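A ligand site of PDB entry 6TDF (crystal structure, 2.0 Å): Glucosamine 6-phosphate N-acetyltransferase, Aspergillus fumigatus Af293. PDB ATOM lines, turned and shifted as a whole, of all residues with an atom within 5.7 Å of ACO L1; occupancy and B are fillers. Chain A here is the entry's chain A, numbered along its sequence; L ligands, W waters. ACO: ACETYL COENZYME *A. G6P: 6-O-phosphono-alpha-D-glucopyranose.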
ATOM      1  N   VAL A  68       0.291 -17.010   1.382  1.00  0.00           N
ATOM      2  CA  VAL A  68       0.265 -17.963   0.229  1.00  0.00           C
ATOM      3  C   VAL A  68      -0.546 -17.364  -0.919  1.00  0.00           C
ATOM      4  O   VAL A  68      -0.465 -17.893  -2.020  1.00  0.00           O
ATOM      5  CB  VAL A  68      -0.294 -19.351   0.611  1.00  0.00           C
ATOM      6  CG1 VAL A  68       0.330 -19.887   1.889  1.00  0.00           C
ATOM      7  CG2 VAL A  68      -1.815 -19.340   0.701  1.00  0.00           C
ATOM      8  N   LEU A  69      -1.361 -16.345  -0.667  1.00  0.00           N
ATOM      9  CA  LEU A  69      -2.341 -15.851  -1.665  1.00  0.00           C
ATOM     10  C   LEU A  69      -1.683 -14.748  -2.486  1.00  0.00           C
ATOM     11  O   LEU A  69      -1.746 -14.787  -3.737  1.00  0.00           O
ATOM     12  CB  LEU A  69      -3.579 -15.346  -0.923  1.00  0.00           C
ATOM     13  CG  LEU A  69      -4.728 -14.871  -1.822  1.00  0.00           C
ATOM     14  CD1 LEU A  69      -5.235 -16.017  -2.684  1.00  0.00           C
ATOM     15  CD2 LEU A  69      -5.846 -14.284  -0.979  1.00  0.00           C
ATOM     16  N   ILE A 128     -17.207 -14.699  -2.968  1.00  0.00           N
ATOM     17  CA  ILE A 128     -16.125 -15.448  -2.281  1.00  0.00           C
ATOM     18  C   ILE A 128     -14.769 -14.817  -2.605  1.00  0.00           C
ATOM     19  O   ILE A 128     -14.461 -14.701  -3.807  1.00  0.00           O
ATOM     20  CB  ILE A 128     -16.175 -16.944  -2.630  1.00  0.00           C
ATOM     21  CG1 ILE A 128     -17.277 -17.633  -1.833  1.00  0.00           C
ATOM     22  CG2 ILE A 128     -14.801 -17.576  -2.423  1.00  0.00           C
ATOM     23  CD1 ILE A 128     -17.558 -19.034  -2.246  1.00  0.00           C
ATOM     24  N   GLU A 129     -13.986 -14.502  -1.575  1.00  0.00           N
ATOM     25  CA  GLU A 129     -12.674 -13.818  -1.715  1.00  0.00           C
ATOM     26  C   GLU A 129     -11.635 -14.487  -0.810  1.00  0.00           C
ATOM     27  O   GLU A 129     -12.018 -15.125   0.205  1.00  0.00           O
ATOM     28  CB  GLU A 129     -12.786 -12.349  -1.331  1.00  0.00           C
ATOM     29  CG  GLU A 129     -13.817 -11.581  -2.110  1.00  0.00           C
ATOM     30  CD  GLU A 129     -13.338 -11.008  -3.442  1.00  0.00           C
ATOM     31  OE1 GLU A 129     -12.121 -10.741  -3.607  1.00  0.00           O
ATOM     32  OE2 GLU A 129     -14.195 -10.815  -4.314  1.00  0.00           O
ATOM     33  N   ASP A 130     -10.362 -14.377  -1.191  1.00  0.00           N
ATOM     34  CA  ASP A 130      -9.171 -14.542  -0.329  1.00  0.00           C
ATOM     35  C   ASP A 130      -9.246 -15.924   0.350  1.00  0.00           C
ATOM     36  O   ASP A 130      -9.196 -15.988   1.596  1.00  0.00           O
ATOM     37  CB  ASP A 130      -9.032 -13.326   0.595  1.00  0.00           C
ATOM     38  CG  ASP A 130      -8.890 -11.994  -0.177  1.00  0.00           C
ATOM     39  OD1 ASP A 130      -8.370 -12.014  -1.298  1.00  0.00           O
ATOM     40  OD2 ASP A 130      -9.291 -10.951   0.361  1.00  0.00           O
ATOM     41  N   ILE A 131      -9.367 -16.979  -0.458  1.00  0.00           N
ATOM     42  CA  ILE A 131      -9.288 -18.404  -0.040  1.00  0.00           C
ATOM     43  C   ILE A 131      -7.797 -18.771  -0.024  1.00  0.00           C
ATOM     44  O   ILE A 131      -7.080 -18.562  -1.032  1.00  0.00           O
ATOM     45  CB  ILE A 131     -10.073 -19.305  -1.000  1.00  0.00           C
ATOM     46  CG1 ILE A 131     -11.507 -18.791  -1.217  1.00  0.00           C
ATOM     47  CG2 ILE A 131     -10.047 -20.756  -0.536  1.00  0.00           C
ATOM     48  CD1 ILE A 131     -12.397 -18.907  -0.021  1.00  0.00           C
ATOM     49  N   ALA A 132      -7.316 -19.240   1.115  1.00  0.00           N
ATOM     50  CA  ALA A 132      -5.897 -19.606   1.300  1.00  0.00           C
ATOM     51  C   ALA A 132      -5.856 -20.800   2.235  1.00  0.00           C
ATOM     52  O   ALA A 132      -6.591 -20.774   3.218  1.00  0.00           O
ATOM     53  CB  ALA A 132      -5.148 -18.441   1.870  1.00  0.00           C
ATOM     54  N   VAL A 133      -5.033 -21.795   1.911  1.00  0.00           N
ATOM     55  CA  VAL A 133      -4.662 -22.905   2.825  1.00  0.00           C
ATOM     56  C   VAL A 133      -3.135 -22.979   2.897  1.00  0.00           C
ATOM     57  O   VAL A 133      -2.488 -23.022   1.808  1.00  0.00           O
ATOM     58  CB  VAL A 133      -5.261 -24.243   2.349  1.00  0.00           C
ATOM     59  CG1 VAL A 133      -4.720 -25.417   3.164  1.00  0.00           C
ATOM     60  CG2 VAL A 133      -6.783 -24.206   2.361  1.00  0.00           C
ATOM     61  N   GLU A 134      -2.591 -22.970   4.112  1.00  0.00           N
ATOM     62  CA  GLU A 134      -1.144 -23.196   4.405  1.00  0.00           C
ATOM     63  C   GLU A 134      -0.587 -24.344   3.546  1.00  0.00           C
ATOM     64  O   GLU A 134      -1.215 -25.432   3.531  1.00  0.00           O
ATOM     65  CB  GLU A 134      -1.039 -23.513   5.894  1.00  0.00           C
ATOM     66  CG  GLU A 134       0.365 -23.756   6.402  1.00  0.00           C
ATOM     67  CD  GLU A 134       0.370 -23.935   7.909  1.00  0.00           C
ATOM     68  OE1 GLU A 134       0.228 -22.910   8.607  1.00  0.00           O
ATOM     69  OE2 GLU A 134       0.433 -25.106   8.375  1.00  0.00           O
ATOM     70  N   GLN A 137      -0.521 -27.900   4.408  1.00  0.00           N
ATOM     71  CA  GLN A 137      -1.892 -28.385   4.699  1.00  0.00           C
ATOM     72  C   GLN A 137      -2.751 -28.482   3.429  1.00  0.00           C
ATOM     73  O   GLN A 137      -3.941 -28.832   3.543  1.00  0.00           O
ATOM     74  CB  GLN A 137      -2.551 -27.449   5.723  1.00  0.00           C
ATOM     75  CG  GLN A 137      -1.868 -27.483   7.072  1.00  0.00           C
ATOM     76  CD  GLN A 137      -2.130 -28.801   7.746  1.00  0.00           C
ATOM     77  OE1 GLN A 137      -3.257 -29.098   8.106  1.00  0.00           O
ATOM     78  NE2 GLN A 137      -1.102 -29.619   7.861  1.00  0.00           N
ATOM     79  N   GLN A 138      -2.197 -28.196   2.258  1.00  0.00           N
ATOM     80  CA  GLN A 138      -2.963 -28.242   0.988  1.00  0.00           C
ATOM     81  C   GLN A 138      -3.181 -29.697   0.605  1.00  0.00           C
ATOM     82  O   GLN A 138      -2.434 -30.561   1.099  1.00  0.00           O
ATOM     83  CB  GLN A 138      -2.264 -27.437  -0.115  1.00  0.00           C
ATOM     84  CG  GLN A 138      -2.350 -25.941   0.139  1.00  0.00           C
ATOM     85  CD  GLN A 138      -1.593 -25.147  -0.901  1.00  0.00           C
ATOM     86  OE1 GLN A 138      -1.145 -25.699  -1.900  1.00  0.00           O
ATOM     87  NE2 GLN A 138      -1.447 -23.854  -0.665  1.00  0.00           N
ATOM     88  N   GLY A 139      -4.223 -29.942  -0.191  1.00  0.00           N
ATOM     89  CA  GLY A 139      -4.510 -31.260  -0.802  1.00  0.00           C
ATOM     90  C   GLY A 139      -5.205 -32.190   0.159  1.00  0.00           C
ATOM     91  O   GLY A 139      -5.193 -33.380  -0.133  1.00  0.00           O
ATOM     92  N   LYS A 140      -5.836 -31.671   1.211  1.00  0.00           N
ATOM     93  CA  LYS A 140      -6.542 -32.459   2.265  1.00  0.00           C
ATOM     94  C   LYS A 140      -8.030 -32.092   2.335  1.00  0.00           C
ATOM     95  O   LYS A 140      -8.638 -32.383   3.381  1.00  0.00           O
ATOM     96  CB  LYS A 140      -5.956 -32.201   3.662  1.00  0.00           C
ATOM     97  CG  LYS A 140      -4.501 -32.550   3.898  1.00  0.00           C
ATOM     98  CD  LYS A 140      -4.079 -32.134   5.313  1.00  0.00           C
ATOM     99  CE  LYS A 140      -2.725 -32.670   5.748  1.00  0.00           C
ATOM    100  NZ  LYS A 140      -1.671 -32.349   4.765  1.00  0.00           N
ATOM    101  N   LYS A 141      -8.599 -31.436   1.309  1.00  0.00           N
ATOM    102  CA  LYS A 141     -10.025 -31.024   1.276  1.00  0.00           C
ATOM    103  C   LYS A 141     -10.308 -29.774   2.120  1.00  0.00           C
ATOM    104  O   LYS A 141     -11.482 -29.410   2.226  1.00  0.00           O
ATOM    105  CB  LYS A 141     -10.921 -32.154   1.777  1.00  0.00           C
ATOM    106  CG  LYS A 141     -10.840 -33.445   0.973  1.00  0.00           C
ATOM    107  CD  LYS A 141     -11.418 -33.302  -0.393  1.00  0.00           C
ATOM    108  CE  LYS A 141     -11.715 -34.644  -1.042  1.00  0.00           C
ATOM    109  NZ  LYS A 141     -10.468 -35.402  -1.289  1.00  0.00           N
ATOM    110  N   LEU A 142      -9.308 -29.130   2.723  1.00  0.00           N
ATOM    111  CA  LEU A 142      -9.572 -27.955   3.606  1.00  0.00           C
ATOM    112  C   LEU A 142     -10.140 -26.819   2.756  1.00  0.00           C
ATOM    113  O   LEU A 142     -11.100 -26.189   3.214  1.00  0.00           O
ATOM    114  CB  LEU A 142      -8.300 -27.527   4.335  1.00  0.00           C
ATOM    115  CG  LEU A 142      -7.693 -28.530   5.315  1.00  0.00           C
ATOM    116  CD1 LEU A 142      -6.545 -27.867   6.067  1.00  0.00           C
ATOM    117  CD2 LEU A 142      -8.724 -29.109   6.278  1.00  0.00           C
ATOM    118  N   GLY A 143      -9.600 -26.597   1.557  1.00  0.00           N
ATOM    119  CA  GLY A 143     -10.140 -25.620   0.592  1.00  0.00           C
ATOM    120  C   GLY A 143     -11.589 -25.889   0.254  1.00  0.00           C
ATOM    121  O   GLY A 143     -12.377 -24.930   0.259  1.00  0.00           O
ATOM    122  N   LEU A 144     -11.936 -27.151  -0.046  1.00  0.00           N
ATOM    123  CA  LEU A 144     -13.325 -27.565  -0.326  1.00  0.00           C
ATOM    124  C   LEU A 144     -14.256 -27.271   0.866  1.00  0.00           C
ATOM    125  O   LEU A 144     -15.421 -26.871   0.627  1.00  0.00           O
ATOM    126  CB  LEU A 144     -13.348 -29.068  -0.663  1.00  0.00           C
ATOM    127  CG  LEU A 144     -14.735 -29.697  -0.667  1.00  0.00           C
ATOM    128  CD1 LEU A 144     -15.594 -29.160  -1.818  1.00  0.00           C
ATOM    129  CD2 LEU A 144     -14.645 -31.219  -0.734  1.00  0.00           C
ATOM    130  N   ARG A 145     -13.819 -27.578   2.087  1.00  0.00           N
ATOM    131  CA  ARG A 145     -14.650 -27.363   3.289  1.00  0.00           C
ATOM    132  C   ARG A 145     -14.868 -25.860   3.444  1.00  0.00           C
ATOM    133  O   ARG A 145     -15.996 -25.450   3.734  1.00  0.00           O
ATOM    134  CB  ARG A 145     -13.973 -27.970   4.517  1.00  0.00           C
ATOM    135  CG  ARG A 145     -13.758 -29.475   4.434  1.00  0.00           C
ATOM    136  CD  ARG A 145     -14.847 -30.193   3.674  1.00  0.00           C
ATOM    137  NE  ARG A 145     -14.633 -31.643   3.692  1.00  0.00           N
ATOM    138  CZ  ARG A 145     -15.243 -32.519   2.899  1.00  0.00           C
ATOM    139  NH1 ARG A 145     -16.156 -32.128   2.035  1.00  0.00           N
ATOM    140  NH2 ARG A 145     -14.966 -33.798   3.019  1.00  0.00           N
ATOM    141  N   LEU A 164     -17.272 -15.747  -7.771  1.00  0.00           N
ATOM    142  CA  LEU A 164     -15.854 -15.512  -7.435  1.00  0.00           C
ATOM    143  C   LEU A 164     -15.092 -15.392  -8.763  1.00  0.00           C
ATOM    144  O   LEU A 164     -15.649 -15.750  -9.810  1.00  0.00           O
ATOM    145  CB  LEU A 164     -15.349 -16.678  -6.588  1.00  0.00           C
ATOM    146  CG  LEU A 164     -15.370 -18.053  -7.255  1.00  0.00           C
ATOM    147  CD1 LEU A 164     -14.046 -18.369  -7.935  1.00  0.00           C
ATOM    148  CD2 LEU A 164     -15.691 -19.129  -6.224  1.00  0.00           C
ATOM    149  N   ASP A 165     -13.904 -14.835  -8.675  1.00  0.00           N
ATOM    150  CA  ASP A 165     -12.924 -14.689  -9.761  1.00  0.00           C
ATOM    151  C   ASP A 165     -11.778 -15.671  -9.484  1.00  0.00           C
ATOM    152  O   ASP A 165     -11.327 -15.757  -8.317  1.00  0.00           O
ATOM    153  CB  ASP A 165     -12.445 -13.236  -9.834  1.00  0.00           C
ATOM    154  CG  ASP A 165     -13.549 -12.277 -10.253  1.00  0.00           C
ATOM    155  OD1 ASP A 165     -14.390 -12.686 -11.100  1.00  0.00           O
ATOM    156  OD2 ASP A 165     -13.553 -11.124  -9.741  1.00  0.00           O
ATOM    157  N   CYS A 166     -11.290 -16.350 -10.514  1.00  0.00           N
ATOM    158  CA  CYS A 166     -10.103 -17.219 -10.399  1.00  0.00           C
ATOM    159  C   CYS A 166      -9.258 -17.149 -11.668  1.00  0.00           C
ATOM    160  O   CYS A 166      -9.628 -16.474 -12.625  1.00  0.00           O
ATOM    161  CB  CYS A 166     -10.524 -18.629 -10.053  1.00  0.00           C
ATOM    162  SG  CYS A 166     -11.378 -19.493 -11.385  1.00  0.00           S
ATOM    163  N   ALA A 169      -5.293 -21.546 -13.796  1.00  0.00           N
ATOM    164  CA  ALA A 169      -4.525 -22.521 -12.985  1.00  0.00           C
ATOM    165  C   ALA A 169      -5.381 -23.075 -11.830  1.00  0.00           C
ATOM    166  O   ALA A 169      -5.176 -24.239 -11.440  1.00  0.00           O
ATOM    167  CB  ALA A 169      -3.254 -21.891 -12.474  1.00  0.00           C
ATOM    168  N   ASN A 170      -6.351 -22.322 -11.291  1.00  0.00           N
ATOM    169  CA  ASN A 170      -7.109 -22.880 -10.149  1.00  0.00           C
ATOM    170  C   ASN A 170      -8.583 -23.046 -10.521  1.00  0.00           C
ATOM    171  O   ASN A 170      -9.348 -23.450  -9.632  1.00  0.00           O
ATOM    172  CB  ASN A 170      -6.771 -22.170  -8.829  1.00  0.00           C
ATOM    173  CG  ASN A 170      -7.143 -20.708  -8.799  1.00  0.00           C
ATOM    174  OD1 ASN A 170      -8.017 -20.281  -9.562  1.00  0.00           O
ATOM    175  ND2 ASN A 170      -6.547 -19.963  -7.885  1.00  0.00           N
ATOM    176  N   GLU A 171      -8.957 -22.895 -11.785  1.00  0.00           N
ATOM    177  CA  GLU A 171     -10.377 -23.084 -12.210  1.00  0.00           C
ATOM    178  C   GLU A 171     -10.853 -24.484 -11.792  1.00  0.00           C
ATOM    179  O   GLU A 171     -12.017 -24.613 -11.387  1.00  0.00           O
ATOM    180  CB  GLU A 171     -10.525 -22.871 -13.712  1.00  0.00           C
ATOM    181  CG  GLU A 171     -11.968 -23.008 -14.177  1.00  0.00           C
ATOM    182  CD  GLU A 171     -12.195 -22.891 -15.661  1.00  0.00           C
ATOM    183  OE1 GLU A 171     -11.182 -22.786 -16.420  1.00  0.00           O
ATOM    184  OE2 GLU A 171     -13.387 -22.887 -16.075  1.00  0.00           O
ATOM    185  N   GLY A 172      -9.987 -25.493 -11.910  1.00  0.00           N
ATOM    186  CA  GLY A 172     -10.317 -26.915 -11.684  1.00  0.00           C
ATOM    187  C   GLY A 172     -10.674 -27.199 -10.239  1.00  0.00           C
ATOM    188  O   GLY A 172     -11.466 -28.140 -10.011  1.00  0.00           O
ATOM    189  N   PHE A 173     -10.131 -26.448  -9.286  1.00  0.00           N
ATOM    190  CA  PHE A 173     -10.515 -26.546  -7.853  1.00  0.00           C
ATOM    191  C   PHE A 173     -11.969 -26.113  -7.702  1.00  0.00           C
ATOM    192  O   PHE A 173     -12.773 -26.847  -7.067  1.00  0.00           O
ATOM    193  CB  PHE A 173      -9.565 -25.751  -6.957  1.00  0.00           C
ATOM    194  CG  PHE A 173     -10.100 -25.466  -5.574  1.00  0.00           C
ATOM    195  CD1 PHE A 173     -10.239 -26.484  -4.648  1.00  0.00           C
ATOM    196  CD2 PHE A 173     -10.439 -24.160  -5.208  1.00  0.00           C
ATOM    197  CE1 PHE A 173     -10.754 -26.214  -3.384  1.00  0.00           C
ATOM    198  CE2 PHE A 173     -10.921 -23.892  -3.943  1.00  0.00           C
ATOM    199  CZ  PHE A 173     -11.100 -24.923  -3.035  1.00  0.00           C
ATOM    200  N   TYR A 174     -12.330 -24.976  -8.324  1.00  0.00           N
ATOM    201  CA  TYR A 174     -13.676 -24.355  -8.200  1.00  0.00           C
ATOM    202  C   TYR A 174     -14.710 -25.245  -8.886  1.00  0.00           C
ATOM    203  O   TYR A 174     -15.828 -25.314  -8.404  1.00  0.00           O
ATOM    204  CB  TYR A 174     -13.634 -22.883  -8.653  1.00  0.00           C
ATOM    205  CG  TYR A 174     -12.808 -22.033  -7.710  1.00  0.00           C
ATOM    206  CD1 TYR A 174     -13.222 -21.894  -6.393  1.00  0.00           C
ATOM    207  CD2 TYR A 174     -11.612 -21.440  -8.078  1.00  0.00           C
ATOM    208  CE1 TYR A 174     -12.487 -21.177  -5.474  1.00  0.00           C
ATOM    209  CE2 TYR A 174     -10.857 -20.713  -7.171  1.00  0.00           C
ATOM    210  CZ  TYR A 174     -11.317 -20.577  -5.855  1.00  0.00           C
ATOM    211  OH  TYR A 174     -10.646 -19.912  -4.880  1.00  0.00           O
ATOM    212  N   LYS A 176     -14.488 -28.558  -9.016  1.00  0.00           N
ATOM    213  CA  LYS A 176     -14.627 -29.692  -8.057  1.00  0.00           C
ATOM    214  C   LYS A 176     -15.521 -29.264  -6.871  1.00  0.00           C
ATOM    215  O   LYS A 176     -16.089 -30.159  -6.240  1.00  0.00           O
ATOM    216  CB  LYS A 176     -13.232 -30.150  -7.618  1.00  0.00           C
ATOM    217  CG  LYS A 176     -12.426 -30.898  -8.679  1.00  0.00           C
ATOM    218  CD  LYS A 176     -12.571 -32.408  -8.592  1.00  0.00           C
ATOM    219  CE  LYS A 176     -11.692 -33.187  -9.561  1.00  0.00           C
ATOM    220  NZ  LYS A 176     -10.431 -33.636  -8.918  1.00  0.00           N
ATOM    221  N   CYS A 177     -15.635 -27.956  -6.612  1.00  0.00           N
ATOM    222  CA  CYS A 177     -16.467 -27.348  -5.548  1.00  0.00           C
ATOM    223  C   CYS A 177     -17.918 -27.161  -6.015  1.00  0.00           C
ATOM    224  O   CYS A 177     -18.774 -26.871  -5.159  1.00  0.00           O
ATOM    225  CB  CYS A 177     -15.911 -26.000  -5.094  1.00  0.00           C
ATOM    226  SG  CYS A 177     -14.348 -26.158  -4.194  1.00  0.00           S
HETATM  227  N1A ACO L   1      -6.474 -27.281  -9.898  1.00  0.00           N
HETATM  228  C2A ACO L   1      -7.200 -28.416 -10.016  1.00  0.00           C
HETATM  229  N3A ACO L   1      -7.554 -29.136  -8.942  1.00  0.00           N
HETATM  230  C4A ACO L   1      -7.232 -28.741  -7.682  1.00  0.00           C
HETATM  231  C5A ACO L   1      -6.462 -27.509  -7.509  1.00  0.00           C
HETATM  232  C6A ACO L   1      -6.088 -26.783  -8.714  1.00  0.00           C
HETATM  233  N6A ACO L   1      -5.398 -25.608  -8.595  1.00  0.00           N
HETATM  234  N7A ACO L   1      -6.285 -27.358  -6.177  1.00  0.00           N
HETATM  235  C8A ACO L   1      -6.864 -28.394  -5.526  1.00  0.00           C
HETATM  236  N9A ACO L   1      -7.421 -29.204  -6.437  1.00  0.00           N
HETATM  237  C1B ACO L   1      -8.183 -30.419  -6.179  1.00  0.00           C
HETATM  238  C2B ACO L   1      -7.677 -31.281  -5.040  1.00  0.00           C
HETATM  239  O2B ACO L   1      -6.688 -32.160  -5.546  1.00  0.00           O
HETATM  240  C3B ACO L   1      -8.957 -31.955  -4.567  1.00  0.00           C
HETATM  241  O3B ACO L   1      -9.253 -32.998  -5.455  1.00  0.00           O
HETATM  242  P3B ACO L   1     -10.193 -34.288  -5.154  1.00  0.00           P
HETATM  243  O7A ACO L   1     -11.601 -33.879  -4.765  1.00  0.00           O
HETATM  244  O8A ACO L   1     -10.238 -34.951  -6.510  1.00  0.00           O
HETATM  245  O9A ACO L   1      -9.311 -34.786  -4.053  1.00  0.00           O
HETATM  246  C4B ACO L   1     -10.009 -30.884  -4.781  1.00  0.00           C
HETATM  247  O4B ACO L   1      -9.487 -30.012  -5.815  1.00  0.00           O
HETATM  248  C5B ACO L   1     -10.295 -30.078  -3.514  1.00  0.00           C
HETATM  249  O5B ACO L   1      -9.080 -29.520  -3.065  1.00  0.00           O
HETATM  250  P1A ACO L   1      -8.604 -29.323  -1.548  1.00  0.00           P
HETATM  251  O1A ACO L   1      -7.630 -30.346  -1.063  1.00  0.00           O
HETATM  252  O2A ACO L   1      -9.800 -28.876  -0.782  1.00  0.00           O
HETATM  253  O3A ACO L   1      -7.597 -28.103  -1.882  1.00  0.00           O
HETATM  254  P2A ACO L   1      -6.582 -27.263  -0.978  1.00  0.00           P
HETATM  255  O4A ACO L   1      -5.218 -27.222  -1.529  1.00  0.00           O
HETATM  256  O5A ACO L   1      -6.882 -27.552   0.465  1.00  0.00           O
HETATM  257  O6A ACO L   1      -7.126 -25.796  -1.314  1.00  0.00           O
HETATM  258  CBP ACO L   1      -6.620 -23.876  -2.580  1.00  0.00           C
HETATM  259  CCP ACO L   1      -7.164 -25.295  -2.635  1.00  0.00           C
HETATM  260  CDP ACO L   1      -7.532 -23.054  -1.684  1.00  0.00           C
HETATM  261  CEP ACO L   1      -6.617 -23.397  -4.019  1.00  0.00           C
HETATM  262  CAP ACO L   1      -5.245 -23.878  -1.935  1.00  0.00           C
HETATM  263  OAP ACO L   1      -4.455 -24.844  -2.640  1.00  0.00           O
HETATM  264  C9P ACO L   1      -4.459 -22.597  -1.932  1.00  0.00           C
HETATM  265  O9P ACO L   1      -4.395 -21.880  -0.953  1.00  0.00           O
HETATM  266  N8P ACO L   1      -3.790 -22.262  -3.032  1.00  0.00           N
HETATM  267  C7P ACO L   1      -3.095 -20.999  -3.061  1.00  0.00           C
HETATM  268  C6P ACO L   1      -3.957 -19.738  -2.959  1.00  0.00           C
HETATM  269  C5P ACO L   1      -5.049 -19.656  -4.016  1.00  0.00           C
HETATM  270  O5P ACO L   1      -4.823 -19.844  -5.186  1.00  0.00           O
HETATM  271  N4P ACO L   1      -6.281 -19.369  -3.604  1.00  0.00           N
HETATM  272  C3P ACO L   1      -7.393 -19.228  -4.520  1.00  0.00           C
HETATM  273  C2P ACO L   1      -7.594 -17.772  -4.999  1.00  0.00           C
HETATM  274  S1P ACO L   1      -9.157 -17.697  -5.874  1.00  0.00           S
HETATM  275  C   ACO L   1     -10.199 -17.027  -4.702  1.00  0.00           C
HETATM  276  O   ACO L   1      -9.748 -16.650  -3.618  1.00  0.00           O
HETATM  277  CH3 ACO L   1     -11.670 -16.916  -4.983  1.00  0.00           C
HETATM  278  C1  G6P L   2      -9.078 -12.273  -4.935  1.00  0.00           C
HETATM  279  C2  G6P L   2      -9.266 -13.071  -6.236  1.00  0.00           C
HETATM  280  C3  G6P L   2      -8.066 -13.887  -6.695  1.00  0.00           C
HETATM  281  C4  G6P L   2      -6.720 -13.237  -6.414  1.00  0.00           C
HETATM  282  C5  G6P L   2      -6.589 -12.642  -5.012  1.00  0.00           C
HETATM  283  C6  G6P L   2      -5.288 -11.830  -4.927  1.00  0.00           C
HETATM  284  O1  G6P L   2      -9.651 -13.061  -3.871  1.00  0.00           O
HETATM  285  O2  G6P L   2     -10.354 -14.007  -6.076  1.00  0.00           O
HETATM  286  O3  G6P L   2      -8.209 -14.148  -8.107  1.00  0.00           O
HETATM  287  O4  G6P L   2      -5.677 -14.237  -6.538  1.00  0.00           O
HETATM  288  O5  G6P L   2      -7.725 -11.838  -4.620  1.00  0.00           O
HETATM  289  O6  G6P L   2      -4.881 -11.248  -6.180  1.00  0.00           O
HETATM  290  P   G6P L   2      -4.346  -9.697  -6.268  1.00  0.00           P
HETATM  291  O1P G6P L   2      -5.586  -8.878  -5.981  1.00  0.00           O
HETATM  292  O2P G6P L   2      -3.784  -9.467  -7.669  1.00  0.00           O
HETATM  293  O3P G6P L   2      -3.273  -9.627  -5.210  1.00  0.00           O
HETATM  294  O   HOH W   1      -6.235 -29.178   2.353  1.00  0.00           O
HETATM  295  O   HOH W   2      -2.863 -28.026  -3.518  1.00  0.00           O
HETATM  296  O   HOH W   3      -6.954 -17.271  -8.371  1.00  0.00           O
HETATM  297  O   HOH W   4      -4.281 -31.301  -4.502  1.00  0.00           O
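Water W2 lies within hydrogen-bond range of O4A of ACO L1 and OE1 of Gln 138.
Water W3 lies within hydrogen-bond range of ND2 of Asn 170 (2.8 Å), S1P of ACO L1 (3.4 Å) and O3 of G6P L2 (3.4 Å).
Val 68 touches ACO L1.
Leu 69 touches ACO L1 (CD1 to N4P, 3.6 Å).
O of Ile 128 touches CH3 of ACO L1, 3.8 Å away.
Ala 132 touches ACO L1 (CA to O9P, 3.5 Å).
N of Leu 142 touches O2A of ACO L1, at 3.5 Å.
Asp 165 touches ACO L1.
Gly 172 touches ACO L1.
Phe 173 touches ACO L1 (N to C2A, 3.6 Å).
Hydrophobic or aromatic side chains within 4 Å of ACO L1: Val 68, Leu 69, Ile 131, Val 133, Leu 144, Phe 173 and Tyr 174.
Of the 29 residues printed, 21 come within 4 Å of ACO L1.
The nearest printed residue that does not touch ACO L1 is Glu 129 (4.02 Å).
NZ of Lys 176 is in salt-bridge range of O8A of ACO L1, at 2.8 Å.
N of Lys 141 is in hydrogen-bond range of O1A of ACO L1 (2.8 Å).
The side-chain amino group (NZ) of Lys 141 lies within salt-bridge range of an oxygen (O9A) of ACO L1 (3.1 Å).
An oxygen (O) of ACO L1 lies within hydrogen-bond range of the backbone NH (N) of Ile 131, 3.2 Å away.
The backbone carbonyl oxygen (O) of Ile 131 sits at hydrogen-bond distance from a nitrogen (N4P) of ACO L1.
The backbone NH (N) of Leu 144 is in hydrogen-bond range of an oxygen (O2A) of ACO L1.
A sulfur (S1P) of ACO L1 sits close to the side-chain hydroxyl (OH) of Tyr 174 (2.8 Å).
The backbone NH (N) of Val 133 lies within hydrogen-bond range of an oxygen (O9P) of ACO L1 (2.9 Å).
The backbone NH (N) of Gly 143 lies within hydrogen-bond range of an oxygen (O5A) of ACO L1 (3.1 Å).
O of Ala 169 lies within hydrogen-bond range of N6A of ACO L1 (3.2 Å).
The backbone NH (N) of Lys 140 is in hydrogen-bond range of an oxygen (O1A) of ACO L1.
The backbone NH of Gly 139 sits at hydrogen-bond distance from an oxygen (O4A) of ACO L1, at 3.2 Å.
An oxygen (O5P) of ACO L1 is in hydrogen-bond range of the side-chain amide nitrogen of Asn 170 (3.2 Å).
The side-chain amide oxygen (OE1) of Gln 138 lies close to an oxygen (OAP) of ACO L1 (3.5 Å).
The backbone NH (N) of Asp 130 lies within hydrogen-bond range of an oxygen (O) of ACO L1 (3.4 Å).
An oxygen (O1) of G6P L2 lies within hydrogen-bond range of the backbone NH of Asp 130 (3.1 Å).
OD1 of Asp 130 sits at hydrogen-bond distance from O1 of G6P L2 (3.1 Å).
O of Asp 165 is in hydrogen-bond range of O2 of G6P L2 (3.0 Å).
OE1 of Glu 129 is in hydrogen-bond range of O1 of G6P L2 (3.4 Å).
O of Val 133 lies within hydrogen-bond range of NE2 of Gln 138 (2.8 Å).
O of Phe 173 is in hydrogen-bond range of SG of Cys 177, at 3.3 Å.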
